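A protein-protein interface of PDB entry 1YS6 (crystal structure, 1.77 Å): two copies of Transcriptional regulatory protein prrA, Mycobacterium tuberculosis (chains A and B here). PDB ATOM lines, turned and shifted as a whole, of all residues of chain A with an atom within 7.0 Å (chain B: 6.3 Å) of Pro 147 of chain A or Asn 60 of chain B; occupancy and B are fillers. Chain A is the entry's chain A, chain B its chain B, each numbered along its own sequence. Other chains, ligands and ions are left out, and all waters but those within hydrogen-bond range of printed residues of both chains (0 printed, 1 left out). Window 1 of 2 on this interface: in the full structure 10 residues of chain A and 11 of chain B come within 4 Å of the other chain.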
ATOM      1  N   SER A 132     -24.593  16.527 -17.130  1.00  0.00           N
ATOM      2  CA  SER A 132     -25.526  17.572 -16.724  1.00  0.00           C
ATOM      3  C   SER A 132     -25.205  18.900 -17.407  1.00  0.00           C
ATOM      4  O   SER A 132     -24.051  19.141 -17.791  1.00  0.00           O
ATOM      5  CB  SER A 132     -25.396  17.798 -15.217  1.00  0.00           C
ATOM      6  OG  SER A 132     -26.247  18.856 -14.838  1.00  0.00           O
ATOM      7  N   SER A 133     -26.214  19.753 -17.601  1.00  0.00           N
ATOM      8  CA  SER A 133     -25.910  21.111 -18.060  1.00  0.00           C
ATOM      9  C   SER A 133     -25.742  22.038 -16.847  1.00  0.00           C
ATOM     10  O   SER A 133     -25.550  23.217 -16.987  1.00  0.00           O
ATOM     11  CB  SER A 133     -26.890  21.651 -19.149  1.00  0.00           C
ATOM     12  OG  SER A 133     -28.059  22.175 -18.535  1.00  0.00           O
ATOM     13  N   SER A 134     -25.865  21.503 -15.620  1.00  0.00           N
ATOM     14  CA  SER A 134     -25.750  22.362 -14.458  1.00  0.00           C
ATOM     15  C   SER A 134     -24.323  22.765 -14.149  1.00  0.00           C
ATOM     16  O   SER A 134     -23.411  21.987 -14.360  1.00  0.00           O
ATOM     17  CB  SER A 134     -26.253  21.551 -13.256  1.00  0.00           C
ATOM     18  OG  SER A 134     -27.575  21.250 -13.601  1.00  0.00           O
ATOM     19  N   GLU A 135     -24.140  24.005 -13.676  1.00  0.00           N
ATOM     20  CA  GLU A 135     -22.822  24.506 -13.309  1.00  0.00           C
ATOM     21  C   GLU A 135     -22.774  24.526 -11.796  1.00  0.00           C
ATOM     22  O   GLU A 135     -22.744  23.433 -11.174  1.00  0.00           O
ATOM     23  CB  GLU A 135     -22.571  25.908 -13.949  1.00  0.00           C
ATOM     24  CG  GLU A 135     -22.932  25.885 -15.434  1.00  0.00           C
ATOM     25  CD  GLU A 135     -22.826  27.233 -16.126  1.00  0.00           C
ATOM     26  OE1 GLU A 135     -21.681  27.666 -16.410  1.00  0.00           O
ATOM     27  OE2 GLU A 135     -23.897  27.807 -16.430  1.00  0.00           O
ATOM     28  N   THR A 136     -22.844  25.712 -11.174  1.00  0.00           N
ATOM     29  CA  THR A 136     -22.947  25.721  -9.681  1.00  0.00           C
ATOM     30  C   THR A 136     -24.371  25.890  -9.146  1.00  0.00           C
ATOM     31  O   THR A 136     -25.018  26.909  -9.401  1.00  0.00           O
ATOM     32  CB  THR A 136     -22.026  26.823  -9.053  1.00  0.00           C
ATOM     33  OG1 THR A 136     -20.685  26.495  -9.370  1.00  0.00           O
ATOM     34  CG2 THR A 136     -22.157  26.788  -7.514  1.00  0.00           C
ATOM     35  N   VAL A 144     -22.961  23.810  -4.736  1.00  0.00           N
ATOM     36  CA  VAL A 144     -22.496  22.601  -5.369  1.00  0.00           C
ATOM     37  C   VAL A 144     -22.000  22.909  -6.764  1.00  0.00           C
ATOM     38  O   VAL A 144     -22.805  23.205  -7.632  1.00  0.00           O
ATOM     39  CB  VAL A 144     -23.606  21.550  -5.497  1.00  0.00           C
ATOM     40  CG1 VAL A 144     -23.009  20.263  -5.998  1.00  0.00           C
ATOM     41  CG2 VAL A 144     -24.203  21.282  -4.132  1.00  0.00           C
ATOM     42  N   ASP A 145     -20.691  22.837  -6.935  1.00  0.00           N
ATOM     43  CA  ASP A 145     -20.063  22.986  -8.254  1.00  0.00           C
ATOM     44  C   ASP A 145     -20.145  21.586  -8.883  1.00  0.00           C
ATOM     45  O   ASP A 145     -19.352  20.693  -8.575  1.00  0.00           O
ATOM     46  CB  ASP A 145     -18.637  23.566  -8.140  1.00  0.00           C
ATOM     47  CG  ASP A 145     -17.881  23.550  -9.439  1.00  0.00           C
ATOM     48  OD1 ASP A 145     -18.471  23.087 -10.437  1.00  0.00           O
ATOM     49  OD2 ASP A 145     -16.694  23.999  -9.448  1.00  0.00           O
ATOM     50  N   ILE A 146     -21.135  21.387  -9.763  1.00  0.00           N
ATOM     51  CA  ILE A 146     -21.330  20.047 -10.430  1.00  0.00           C
ATOM     52  C   ILE A 146     -20.119  19.556 -11.246  1.00  0.00           C
ATOM     53  O   ILE A 146     -19.505  18.549 -10.962  1.00  0.00           O
ATOM     54  CB  ILE A 146     -22.705  19.980 -11.214  1.00  0.00           C
ATOM     55  CG1 ILE A 146     -23.896  20.342 -10.347  1.00  0.00           C
ATOM     56  CG2 ILE A 146     -22.951  18.524 -11.785  1.00  0.00           C
ATOM     57  CD1 ILE A 146     -24.244  19.136  -9.543  1.00  0.00           C
ATOM     58  N   PRO A 147     -19.734  20.328 -12.303  1.00  0.00           N
ATOM     59  CA  PRO A 147     -18.658  19.958 -13.184  1.00  0.00           C
ATOM     60  C   PRO A 147     -17.347  19.843 -12.426  1.00  0.00           C
ATOM     61  O   PRO A 147     -16.617  18.910 -12.651  1.00  0.00           O
ATOM     62  CB  PRO A 147     -18.631  21.082 -14.222  1.00  0.00           C
ATOM     63  CG  PRO A 147     -19.546  22.114 -13.739  1.00  0.00           C
ATOM     64  CD  PRO A 147     -20.429  21.548 -12.669  1.00  0.00           C
ATOM     65  N   GLY A 148     -17.092  20.756 -11.476  1.00  0.00           N
ATOM     66  CA  GLY A 148     -15.899  20.707 -10.591  1.00  0.00           C
ATOM     67  C   GLY A 148     -15.954  19.702  -9.434  1.00  0.00           C
ATOM     68  O   GLY A 148     -14.949  19.416  -8.776  1.00  0.00           O
ATOM     69  N   ARG A 149     -17.097  19.078  -9.234  1.00  0.00           N
ATOM     70  CA  ARG A 149     -17.213  18.100  -8.157  1.00  0.00           C
ATOM     71  C   ARG A 149     -16.669  18.699  -6.864  1.00  0.00           C
ATOM     72  O   ARG A 149     -15.852  18.083  -6.178  1.00  0.00           O
ATOM     73  CB  ARG A 149     -16.508  16.758  -8.529  1.00  0.00           C
ATOM     74  CG  ARG A 149     -17.116  16.043  -9.762  1.00  0.00           C
ATOM     75  CD  ARG A 149     -16.654  14.542  -9.938  1.00  0.00           C
ATOM     76  NE  ARG A 149     -16.989  13.698  -8.762  1.00  0.00           N
ATOM     77  CZ  ARG A 149     -18.143  13.073  -8.588  1.00  0.00           C
ATOM     78  NH1 ARG A 149     -19.092  13.190  -9.502  1.00  0.00           N
ATOM     79  NH2 ARG A 149     -18.344  12.348  -7.473  1.00  0.00           N
ATOM     80  N   ARG A 150     -17.111  19.912  -6.562  1.00  0.00           N
ATOM     81  CA  ARG A 150     -16.802  20.576  -5.244  1.00  0.00           C
ATOM     82  C   ARG A 150     -18.081  21.029  -4.562  1.00  0.00           C
ATOM     83  O   ARG A 150     -19.044  21.443  -5.217  1.00  0.00           O
ATOM     84  CB  ARG A 150     -15.836  21.798  -5.383  1.00  0.00           C
ATOM     85  CG  ARG A 150     -16.584  23.180  -5.467  1.00  0.00           C
ATOM     86  CD  ARG A 150     -16.005  24.431  -4.614  1.00  0.00           C
ATOM     87  NE  ARG A 150     -16.581  25.748  -5.002  1.00  0.00           N
ATOM     88  CZ  ARG A 150     -17.875  26.082  -4.893  1.00  0.00           C
ATOM     89  NH1 ARG A 150     -18.766  25.212  -4.400  1.00  0.00           N
ATOM     90  NH2 ARG A 150     -18.295  27.282  -5.289  1.00  0.00           N
ATOM     91  N   PHE A 165     -20.435  12.824  -2.899  1.00  0.00           N
ATOM     92  CA  PHE A 165     -20.727  13.845  -3.893  1.00  0.00           C
ATOM     93  C   PHE A 165     -21.779  13.434  -4.910  1.00  0.00           C
ATOM     94  O   PHE A 165     -22.693  14.222  -5.225  1.00  0.00           O
ATOM     95  CB  PHE A 165     -19.464  14.276  -4.639  1.00  0.00           C
ATOM     96  CG  PHE A 165     -19.717  15.484  -5.466  1.00  0.00           C
ATOM     97  CD1 PHE A 165     -19.604  16.728  -4.883  1.00  0.00           C
ATOM     98  CD2 PHE A 165     -20.140  15.365  -6.792  1.00  0.00           C
ATOM     99  CE1 PHE A 165     -19.914  17.873  -5.591  1.00  0.00           C
ATOM    100  CE2 PHE A 165     -20.447  16.487  -7.543  1.00  0.00           C
ATOM    101  CZ  PHE A 165     -20.343  17.763  -6.939  1.00  0.00           C
ATOM    102  N   GLU A 173     -29.210  18.723  -8.249  1.00  0.00           N
ATOM    103  CA  GLU A 173     -29.818  18.752  -9.590  1.00  0.00           C
ATOM    104  C   GLU A 173     -31.338  18.668  -9.573  1.00  0.00           C
ATOM    105  O   GLU A 173     -32.012  19.203 -10.406  1.00  0.00           O
ATOM    106  CB  GLU A 173     -29.278  17.556 -10.416  1.00  0.00           C
ATOM    107  CG  GLU A 173     -27.796  17.612 -10.664  1.00  0.00           C
ATOM    108  CD  GLU A 173     -27.480  18.387 -11.934  1.00  0.00           C
ATOM    109  OE1 GLU A 173     -28.356  19.146 -12.393  1.00  0.00           O
ATOM    110  OE2 GLU A 173     -26.351  18.257 -12.448  1.00  0.00           O
ATOM    111  N   ASP B  14     -13.262  26.418 -21.601  1.00  0.00           N
ATOM    112  CA  ASP B  14     -13.280  26.224 -20.154  1.00  0.00           C
ATOM    113  C   ASP B  14     -14.571  26.785 -19.622  1.00  0.00           C
ATOM    114  O   ASP B  14     -14.991  27.883 -20.008  1.00  0.00           O
ATOM    115  CB  ASP B  14     -12.115  26.989 -19.500  1.00  0.00           C
ATOM    116  CG  ASP B  14     -11.708  26.384 -18.181  1.00  0.00           C
ATOM    117  OD1 ASP B  14     -12.523  26.430 -17.235  1.00  0.00           O
ATOM    118  OD2 ASP B  14     -10.571  25.912 -18.089  1.00  0.00           O
ATOM    119  N   ASP B  15     -15.185  26.084 -18.624  1.00  0.00           N
ATOM    120  CA  ASP B  15     -16.414  26.585 -18.102  1.00  0.00           C
ATOM    121  C   ASP B  15     -16.196  27.511 -16.898  1.00  0.00           C
ATOM    122  O   ASP B  15     -17.175  27.992 -16.327  1.00  0.00           O
ATOM    123  CB  ASP B  15     -17.294  25.398 -17.634  1.00  0.00           C
ATOM    124  CG  ASP B  15     -16.635  24.605 -16.536  1.00  0.00           C
ATOM    125  OD1 ASP B  15     -15.428  24.324 -16.590  1.00  0.00           O
ATOM    126  OD2 ASP B  15     -17.310  24.267 -15.553  1.00  0.00           O
ATOM    127  N   ASP B  58     -10.664  22.202 -21.571  1.00  0.00           N
ATOM    128  CA  ASP B  58     -10.890  21.793 -20.169  1.00  0.00           C
ATOM    129  C   ASP B  58     -11.655  20.478 -20.236  1.00  0.00           C
ATOM    130  O   ASP B  58     -12.483  20.316 -21.109  1.00  0.00           O
ATOM    131  CB  ASP B  58     -11.710  22.861 -19.481  1.00  0.00           C
ATOM    132  CG  ASP B  58     -11.889  22.587 -18.017  1.00  0.00           C
ATOM    133  OD1 ASP B  58     -11.016  21.994 -17.359  1.00  0.00           O
ATOM    134  OD2 ASP B  58     -12.927  23.038 -17.570  1.00  0.00           O
ATOM    135  N   ILE B  59     -11.424  19.585 -19.271  1.00  0.00           N
ATOM    136  CA  ILE B  59     -12.017  18.246 -19.332  1.00  0.00           C
ATOM    137  C   ILE B  59     -13.414  18.324 -18.688  1.00  0.00           C
ATOM    138  O   ILE B  59     -14.430  17.886 -19.252  1.00  0.00           O
ATOM    139  CB  ILE B  59     -11.124  17.166 -18.646  1.00  0.00           C
ATOM    140  CG1 ILE B  59      -9.822  16.891 -19.406  1.00  0.00           C
ATOM    141  CG2 ILE B  59     -11.889  15.835 -18.479  1.00  0.00           C
ATOM    142  CD1 ILE B  59     -10.038  16.146 -20.691  1.00  0.00           C
ATOM    143  N   ASN B  60     -13.466  18.865 -17.488  1.00  0.00           N
ATOM    144  CA  ASN B  60     -14.714  18.812 -16.711  1.00  0.00           C
ATOM    145  C   ASN B  60     -15.542  20.072 -16.896  1.00  0.00           C
ATOM    146  O   ASN B  60     -15.229  21.144 -16.319  1.00  0.00           O
ATOM    147  CB  ASN B  60     -14.326  18.657 -15.260  1.00  0.00           C
ATOM    148  CG  ASN B  60     -13.606  17.365 -14.996  1.00  0.00           C
ATOM    149  OD1 ASN B  60     -14.160  16.274 -15.195  1.00  0.00           O
ATOM    150  ND2 ASN B  60     -12.366  17.465 -14.532  1.00  0.00           N
ATOM    151  N   MET B  61     -16.575  19.972 -17.733  1.00  0.00           N
ATOM    152  CA  MET B  61     -17.448  21.075 -18.126  1.00  0.00           C
ATOM    153  C   MET B  61     -18.864  20.518 -18.157  1.00  0.00           C
ATOM    154  O   MET B  61     -18.990  19.325 -18.456  1.00  0.00           O
ATOM    155  CB  MET B  61     -17.108  21.467 -19.560  1.00  0.00           C
ATOM    156  CG  MET B  61     -15.788  22.077 -19.637  1.00  0.00           C
ATOM    157  SD  MET B  61     -15.447  22.656 -21.302  1.00  0.00           S
ATOM    158  CE  MET B  61     -15.416  21.113 -22.187  1.00  0.00           C
ATOM    159  N   PRO B  62     -19.890  21.384 -18.020  1.00  0.00           N
ATOM    160  CA  PRO B  62     -21.281  21.062 -18.177  1.00  0.00           C
ATOM    161  C   PRO B  62     -21.596  20.817 -19.641  1.00  0.00           C
ATOM    162  O   PRO B  62     -20.764  21.107 -20.529  1.00  0.00           O
ATOM    163  CB  PRO B  62     -22.010  22.321 -17.751  1.00  0.00           C
ATOM    164  CG  PRO B  62     -21.028  23.340 -17.490  1.00  0.00           C
ATOM    165  CD  PRO B  62     -19.691  22.847 -17.867  1.00  0.00           C
ATOM    166  N   ASP B  65     -18.714  17.262 -21.775  1.00  0.00           N
ATOM    167  CA  ASP B  65     -17.344  17.370 -21.205  1.00  0.00           C
ATOM    168  C   ASP B  65     -16.220  17.304 -22.229  1.00  0.00           C
ATOM    169  O   ASP B  65     -16.483  17.086 -23.424  1.00  0.00           O
ATOM    170  CB  ASP B  65     -17.098  16.517 -19.962  1.00  0.00           C
ATOM    171  CG  ASP B  65     -17.083  15.014 -20.232  1.00  0.00           C
ATOM    172  OD1 ASP B  65     -16.708  14.586 -21.324  1.00  0.00           O
ATOM    173  OD2 ASP B  65     -17.374  14.238 -19.290  1.00  0.00           O
ATOM    174  N   GLY B  66     -14.980  17.494 -21.768  1.00  0.00           N
ATOM    175  CA  GLY B  66     -13.830  17.584 -22.703  1.00  0.00           C
ATOM    176  C   GLY B  66     -13.598  16.224 -23.350  1.00  0.00           C
ATOM    177  O   GLY B  66     -13.275  16.128 -24.526  1.00  0.00           O
ATOM    178  N   LEU B  85      -6.938  20.275 -20.470  1.00  0.00           N
ATOM    179  CA  LEU B  85      -6.612  20.814 -19.154  1.00  0.00           C
ATOM    180  C   LEU B  85      -7.403  20.062 -18.127  1.00  0.00           C
ATOM    181  O   LEU B  85      -8.576  19.756 -18.376  1.00  0.00           O
ATOM    182  CB  LEU B  85      -7.014  22.300 -19.102  1.00  0.00           C
ATOM    183  CG  LEU B  85      -6.585  23.284 -20.200  1.00  0.00           C
ATOM    184  CD1 LEU B  85      -7.043  24.710 -19.818  1.00  0.00           C
ATOM    185  CD2 LEU B  85      -5.068  23.233 -20.457  1.00  0.00           C
ATOM    186  N   SER B  86      -6.790  19.803 -16.959  1.00  0.00           N
ATOM    187  CA  SER B  86      -7.531  19.294 -15.812  1.00  0.00           C
ATOM    188  C   SER B  86      -6.963  19.787 -14.510  1.00  0.00           C
ATOM    189  O   SER B  86      -5.780  20.123 -14.438  1.00  0.00           O
ATOM    190  CB  SER B  86      -7.595  17.771 -15.842  1.00  0.00           C
ATOM    191  OG  SER B  86      -6.355  17.195 -15.475  1.00  0.00           O
ATOM    192  N   ALA B  87      -7.804  19.819 -13.465  1.00  0.00           N
ATOM    193  CA  ALA B  87      -7.312  20.045 -12.106  1.00  0.00           C
ATOM    194  C   ALA B  87      -6.327  18.951 -11.759  1.00  0.00           C
ATOM    195  O   ALA B  87      -6.370  17.875 -12.359  1.00  0.00           O
ATOM    196  CB  ALA B  87      -8.479  20.053 -11.078  1.00  0.00           C
ATOM    197  N   SER B  90      -7.909  15.446 -10.670  1.00  0.00           N
ATOM    198  CA  SER B  90      -8.756  14.830 -11.698  1.00  0.00           C
ATOM    199  C   SER B  90      -7.965  13.967 -12.736  1.00  0.00           C
ATOM    200  O   SER B  90      -8.114  14.095 -13.963  1.00  0.00           O
ATOM    201  CB  SER B  90      -9.601  15.923 -12.348  1.00  0.00           C
ATOM    202  OG  SER B  90     -10.561  15.397 -13.265  1.00  0.00           O
ATOM    203  N   ASP B  93      -9.272  10.290 -15.789  1.00  0.00           N
ATOM    204  CA  ASP B  93     -10.159  11.364 -16.182  1.00  0.00           C
ATOM    205  C   ASP B  93      -9.486  12.359 -17.218  1.00  0.00           C
ATOM    206  O   ASP B  93      -9.944  12.483 -18.380  1.00  0.00           O
ATOM    207  CB  ASP B  93     -10.668  12.072 -14.912  1.00  0.00           C
ATOM    208  CG  ASP B  93     -11.838  13.054 -15.180  1.00  0.00           C
ATOM    209  OD1 ASP B  93     -12.610  13.354 -14.243  1.00  0.00           O
ATOM    210  OD2 ASP B  93     -11.960  13.547 -16.316  1.00  0.00           O
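The side-chain carboxylate (OD1) of Asp 93 of chain B sits close to the side-chain amide oxygen (OD1) of Asn 60 of chain B, at 3.4 Å.
The side-chain hydroxyl (OG) of Ser 132 of chain A sits at hydrogen-bond distance from the backbone NH (N) of Ser 134 of chain A (2.8 Å).
N of Ile 146 of chain A is in hydrogen-bond range of O of Glu 135 of chain A (3.0 Å).
OG of Ser 132 of chain A lies within hydrogen-bond range of OE2 of Glu 173 of chain A (2.5 Å).
The side-chain amide nitrogen (ND2) of Asn 60 of chain B sits at hydrogen-bond distance from the side-chain hydroxyl (OG) of Ser 90 of chain B.
OG of Ser 134 of chain A sits at hydrogen-bond distance from OE1 of Glu 173 of chain A (2.5 Å).
Among the printed residues, merely in contact across the chains: Ser 132 of chain A with Pro 62 of chain B, Pro 147 of chain A with Asn 60 of chain B, Pro 147 of chain A with Asp 15 of chain B, Ser 134 of chain A with Pro 62 of chain B, Ser 133 of chain A with Pro 62 of chain B, Glu 135 of chain A with Pro 62 of chain B and Pro 147 of chain A with Met 61 of chain B.
Printed residues of chain B within 4 Å of Pro 147 of chain A: Asp 15, Asn 60 and Met 61.
Asn 60 of chain B touches one residue of chain A.
Of the printed residues of chain B, Ser 132 of chain A touches Pro 62.
Of the printed residues of chain A, Asp 15 of chain B touches Pro 147 (3.6 Å).
Of the printed residues of chain A, Pro 62 of chain B touches Ser 132, Ser 133, Ser 134 and Glu 135.
Of the printed residues of chain B, Ser 133 of chain A touches Pro 62 (3.7 Å).
Gly 66 of chain B touches none of the printed residues of chain A.
Ser 90 of chain B touches none of the printed residues of chain A.
The nearest printed residue of chain B that does not touch Pro 147 of chain A is Pro 62 of chain B (4.01 Å).
The nearest residue of chain A that does not touch Asn 60 of chain B is Gly 148 of chain A (5.1 Å).
Hydrophobic or aromatic side chains of chain B within 4 Å of the printed part of chain A: Pro 62.
Hydrophobic or aromatic side chains of chain A within 4 Å of the printed part of chain B: Pro 147.
Among the printed residues, no Asp or Glu carboxylate lies within 4 Å of a Lys or Arg side-chain nitrogen of the other chain.
No position is printed for both chains.
Of the 7 pairs that touch across the chains among the printed residues, none has its exchanged pair printed and touching as well.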
